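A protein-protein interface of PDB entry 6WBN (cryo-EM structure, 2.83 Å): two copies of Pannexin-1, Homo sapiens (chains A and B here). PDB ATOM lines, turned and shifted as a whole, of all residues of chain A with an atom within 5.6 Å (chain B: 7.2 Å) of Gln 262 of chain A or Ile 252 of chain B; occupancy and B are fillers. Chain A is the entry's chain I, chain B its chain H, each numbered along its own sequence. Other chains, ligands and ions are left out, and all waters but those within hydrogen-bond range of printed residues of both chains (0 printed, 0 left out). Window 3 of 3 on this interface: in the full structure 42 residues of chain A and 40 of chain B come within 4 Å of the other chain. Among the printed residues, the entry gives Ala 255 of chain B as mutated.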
ATOM      1  N   VAL A 245      31.192  -2.389  13.858  1.00  0.00           N
ATOM      2  CA  VAL A 245      30.208  -1.599  13.137  1.00  0.00           C
ATOM      3  C   VAL A 245      30.758  -1.270  11.762  1.00  0.00           C
ATOM      4  O   VAL A 245      31.879  -0.771  11.637  1.00  0.00           O
ATOM      5  CB  VAL A 245      29.864  -0.325  13.912  1.00  0.00           C
ATOM      6  CG1 VAL A 245      28.742   0.375  13.255  1.00  0.00           C
ATOM      7  CG2 VAL A 245      29.487  -0.676  15.322  1.00  0.00           C
ATOM      8  N   CYS A 246      29.971  -1.531  10.730  1.00  0.00           N
ATOM      9  CA  CYS A 246      30.408  -1.396   9.351  1.00  0.00           C
ATOM     10  C   CYS A 246      29.450  -0.482   8.609  1.00  0.00           C
ATOM     11  O   CYS A 246      28.256  -0.454   8.910  1.00  0.00           O
ATOM     12  CB  CYS A 246      30.480  -2.764   8.685  1.00  0.00           C
ATOM     13  SG  CYS A 246      30.418  -2.785   6.901  1.00  0.00           S
ATOM     14  N   SER A 247      29.972   0.279   7.651  1.00  0.00           N
ATOM     15  CA  SER A 247      29.192   1.292   6.949  1.00  0.00           C
ATOM     16  C   SER A 247      29.431   1.185   5.452  1.00  0.00           C
ATOM     17  O   SER A 247      30.547   1.419   4.984  1.00  0.00           O
ATOM     18  CB  SER A 247      29.557   2.684   7.436  1.00  0.00           C
ATOM     19  OG  SER A 247      30.904   2.966   7.124  1.00  0.00           O
ATOM     20  N   PRO A 260      21.050   2.724   5.983  1.00  0.00           N
ATOM     21  CA  PRO A 260      21.405   3.267   7.292  1.00  0.00           C
ATOM     22  C   PRO A 260      22.874   3.632   7.356  1.00  0.00           C
ATOM     23  O   PRO A 260      23.687   3.217   6.533  1.00  0.00           O
ATOM     24  CB  PRO A 260      21.077   2.120   8.248  1.00  0.00           C
ATOM     25  CG  PRO A 260      21.052   0.918   7.402  1.00  0.00           C
ATOM     26  CD  PRO A 260      20.543   1.355   6.079  1.00  0.00           C
ATOM     27  N   ASP A 261      23.209   4.442   8.357  1.00  0.00           N
ATOM     28  CA  ASP A 261      24.564   4.962   8.445  1.00  0.00           C
ATOM     29  C   ASP A 261      25.564   3.859   8.735  1.00  0.00           C
ATOM     30  O   ASP A 261      26.709   3.924   8.283  1.00  0.00           O
ATOM     31  CB  ASP A 261      24.643   6.052   9.506  1.00  0.00           C
ATOM     32  CG  ASP A 261      24.026   7.346   9.044  1.00  0.00           C
ATOM     33  OD1 ASP A 261      24.047   7.604   7.824  1.00  0.00           O
ATOM     34  OD2 ASP A 261      23.528   8.110   9.896  1.00  0.00           O
ATOM     35  N   GLN A 262      25.161   2.846   9.497  1.00  0.00           N
ATOM     36  CA  GLN A 262      26.092   1.804   9.886  1.00  0.00           C
ATOM     37  C   GLN A 262      25.340   0.542  10.275  1.00  0.00           C
ATOM     38  O   GLN A 262      24.189   0.595  10.706  1.00  0.00           O
ATOM     39  CB  GLN A 262      26.973   2.277  11.031  1.00  0.00           C
ATOM     40  CG  GLN A 262      26.228   2.946  12.143  1.00  0.00           C
ATOM     41  CD  GLN A 262      27.163   3.638  13.097  1.00  0.00           C
ATOM     42  OE1 GLN A 262      28.315   3.912  12.759  1.00  0.00           O
ATOM     43  NE2 GLN A 262      26.684   3.920  14.299  1.00  0.00           N
ATOM     44  N   PHE A 263      26.015  -0.594  10.122  1.00  0.00           N
ATOM     45  CA  PHE A 263      25.445  -1.906  10.366  1.00  0.00           C
ATOM     46  C   PHE A 263      26.211  -2.608  11.474  1.00  0.00           C
ATOM     47  O   PHE A 263      27.415  -2.409  11.635  1.00  0.00           O
ATOM     48  CB  PHE A 263      25.494  -2.773   9.120  1.00  0.00           C
ATOM     49  CG  PHE A 263      24.745  -2.213   7.964  1.00  0.00           C
ATOM     50  CD1 PHE A 263      25.312  -1.260   7.159  1.00  0.00           C
ATOM     51  CD2 PHE A 263      23.476  -2.642   7.681  1.00  0.00           C
ATOM     52  CE1 PHE A 263      24.628  -0.746   6.099  1.00  0.00           C
ATOM     53  CE2 PHE A 263      22.790  -2.126   6.623  1.00  0.00           C
ATOM     54  CZ  PHE A 263      23.368  -1.181   5.829  1.00  0.00           C
ATOM     55  N   GLN A 264      25.509  -3.443  12.226  1.00  0.00           N
ATOM     56  CA  GLN A 264      26.123  -4.220  13.298  1.00  0.00           C
ATOM     57  C   GLN A 264      26.483  -5.591  12.755  1.00  0.00           C
ATOM     58  O   GLN A 264      25.625  -6.460  12.623  1.00  0.00           O
ATOM     59  CB  GLN A 264      25.181  -4.343  14.483  1.00  0.00           C
ATOM     60  CG  GLN A 264      25.715  -5.221  15.570  1.00  0.00           C
ATOM     61  CD  GLN A 264      26.929  -4.625  16.210  1.00  0.00           C
ATOM     62  OE1 GLN A 264      26.963  -3.438  16.495  1.00  0.00           O
ATOM     63  NE2 GLN A 264      27.936  -5.444  16.443  1.00  0.00           N
ATOM     64  N   LYS B 249      21.532  -7.536  21.539  1.00  0.00           N
ATOM     65  CA  LYS B 249      21.352  -6.126  21.855  1.00  0.00           C
ATOM     66  C   LYS B 249      22.645  -5.499  22.334  1.00  0.00           C
ATOM     67  O   LYS B 249      22.636  -4.665  23.241  1.00  0.00           O
ATOM     68  CB  LYS B 249      20.261  -5.907  22.898  1.00  0.00           C
ATOM     69  CG  LYS B 249      18.898  -6.404  22.483  1.00  0.00           C
ATOM     70  CD  LYS B 249      18.237  -5.470  21.505  1.00  0.00           C
ATOM     71  CE  LYS B 249      17.380  -4.457  22.218  1.00  0.00           C
ATOM     72  NZ  LYS B 249      16.493  -3.751  21.269  1.00  0.00           N
ATOM     73  N   SER B 250      23.761  -5.904  21.762  1.00  0.00           N
ATOM     74  CA  SER B 250      25.025  -5.241  22.017  1.00  0.00           C
ATOM     75  C   SER B 250      25.325  -4.269  20.891  1.00  0.00           C
ATOM     76  O   SER B 250      24.838  -4.412  19.769  1.00  0.00           O
ATOM     77  CB  SER B 250      26.154  -6.260  22.155  1.00  0.00           C
ATOM     78  OG  SER B 250      25.955  -7.074  23.294  1.00  0.00           O
ATOM     79  N   GLY B 251      26.127  -3.263  21.205  1.00  0.00           N
ATOM     80  CA  GLY B 251      26.485  -2.337  20.160  1.00  0.00           C
ATOM     81  C   GLY B 251      25.317  -1.448  19.778  1.00  0.00           C
ATOM     82  O   GLY B 251      24.465  -1.100  20.597  1.00  0.00           O
ATOM     83  N   ILE B 252      25.277  -1.079  18.498  1.00  0.00           N
ATOM     84  CA  ILE B 252      24.269  -0.145  18.024  1.00  0.00           C
ATOM     85  C   ILE B 252      22.874  -0.737  18.005  1.00  0.00           C
ATOM     86  O   ILE B 252      21.904   0.006  17.848  1.00  0.00           O
ATOM     87  CB  ILE B 252      24.632   0.362  16.619  1.00  0.00           C
ATOM     88  CG1 ILE B 252      24.428  -0.741  15.599  1.00  0.00           C
ATOM     89  CG2 ILE B 252      26.058   0.819  16.590  1.00  0.00           C
ATOM     90  CD1 ILE B 252      24.641  -0.293  14.200  1.00  0.00           C
ATOM     91  N   LEU B 253      22.738  -2.047  18.153  1.00  0.00           N
ATOM     92  CA  LEU B 253      21.404  -2.618  18.229  1.00  0.00           C
ATOM     93  C   LEU B 253      20.755  -2.395  19.578  1.00  0.00           C
ATOM     94  O   LEU B 253      19.575  -2.714  19.738  1.00  0.00           O
ATOM     95  CB  LEU B 253      21.442  -4.112  17.935  1.00  0.00           C
ATOM     96  CG  LEU B 253      21.690  -4.468  16.479  1.00  0.00           C
ATOM     97  CD1 LEU B 253      21.590  -5.951  16.300  1.00  0.00           C
ATOM     98  CD2 LEU B 253      20.696  -3.761  15.612  1.00  0.00           C
ATOM     99  N   ARG B 254      21.496  -1.871  20.548  1.00  0.00           N
ATOM    100  CA  ARG B 254      20.924  -1.606  21.858  1.00  0.00           C
ATOM    101  C   ARG B 254      19.804  -0.587  21.755  1.00  0.00           C
ATOM    102  O   ARG B 254      18.771  -0.709  22.420  1.00  0.00           O
ATOM    103  CB  ARG B 254      22.014  -1.117  22.799  1.00  0.00           C
ATOM    104  CG  ARG B 254      21.607  -1.074  24.237  1.00  0.00           C
ATOM    105  CD  ARG B 254      22.816  -0.786  25.093  1.00  0.00           C
ATOM    106  NE  ARG B 254      23.833  -1.818  24.931  1.00  0.00           N
ATOM    107  CZ  ARG B 254      24.990  -1.630  24.307  1.00  0.00           C
ATOM    108  NH1 ARG B 254      25.855  -2.627  24.200  1.00  0.00           N
ATOM    109  NH2 ARG B 254      25.282  -0.445  23.789  1.00  0.00           N
ATOM    110  N   ALA B 255      20.021   0.427  20.910  1.00  0.00           N
ATOM    111  CA  ALA B 255      19.040   1.518  20.706  1.00  0.00           C
ATOM    112  C   ALA B 255      17.966   1.089  19.701  1.00  0.00           C
ATOM    113  O   ALA B 255      16.953   1.806  19.581  1.00  0.00           O
ATOM    114  CB  ALA B 255      19.753   2.769  20.252  1.00  0.00           C
ATOM    115  N   ASP B 256      18.162  -0.045  19.016  1.00  0.00           N
ATOM    116  CA  ASP B 256      17.206  -0.552  17.987  1.00  0.00           C
ATOM    117  C   ASP B 256      15.933  -1.096  18.652  1.00  0.00           C
ATOM    118  O   ASP B 256      16.038  -2.073  19.414  1.00  0.00           O
ATOM    119  CB  ASP B 256      17.861  -1.615  17.105  1.00  0.00           C
ATOM    120  CG  ASP B 256      17.368  -1.606  15.669  1.00  0.00           C
ATOM    121  OD1 ASP B 256      16.146  -1.478  15.471  1.00  0.00           O
ATOM    122  OD2 ASP B 256      18.211  -1.733  14.760  1.00  0.00           O
ATOM    123  N   SER B 257      14.775  -0.492  18.354  1.00  0.00           N
ATOM    124  CA  SER B 257      13.481  -0.915  18.959  1.00  0.00           C
ATOM    125  C   SER B 257      12.744  -1.958  18.104  1.00  0.00           C
ATOM    126  O   SER B 257      11.745  -2.509  18.601  1.00  0.00           O
ATOM    127  CB  SER B 257      12.605   0.278  19.244  1.00  0.00           C
ATOM    128  OG  SER B 257      11.686   0.495  18.185  1.00  0.00           O
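O of Gly 251 of chain B sits close to NH2 of Arg 254 of chain B, at 3.4 Å.
The backbone carbonyl oxygen (O) of Cys 246 of chain A is in hydrogen-bond range of the backbone NH (N) of Phe 263 of chain A.
No position is printed for both chains.
Hydrophobic or aromatic side chains of chain A within 4 Å of the printed part of chain B: Val 245.
Printed residues of chain B that touch a printed residue of chain A: Gly 251 and Ile 252.
Among the printed residues, 5 pairs touch across the chains.
Among the printed residues, no Asp or Glu carboxylate lies within 4 Å of a Lys or Arg side-chain nitrogen of the other chain.
Among the printed residues, merely in contact across the chains: Val 245 of chain A with Ile 252 of chain B, Gln 262 of chain A with Ile 252 of chain B, Phe 263 of chain A with Ile 252 of chain B, Gln 264 of chain A with Gly 251 of chain B and Gln 264 of chain A with Ile 252 of chain B.
Of the printed residues of chain B, Val 245 of chain A touches Ile 252.
Gln 262 of chain A touches one residue of chain B.
Printed residues of chain B within 4 Å of Gln 264 of chain A: Gly 251 (3.9 Å) and Ile 252 (3.5 Å).
Of the printed residues of chain A, Gly 251 of chain B touches Gln 264 (3.9 Å).
Of chain A, only Val 245, Gln 262, Phe 263 and Gln 264 come within 4 Å of Ile 252 of chain B.
The nearest printed residue of chain B that does not touch Gln 262 of chain A is Leu 253 of chain B (7.4 Å).
The nearest printed residue of chain B that does not touch Gln 264 of chain A is Ser 250 of chain B (4.02 Å).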
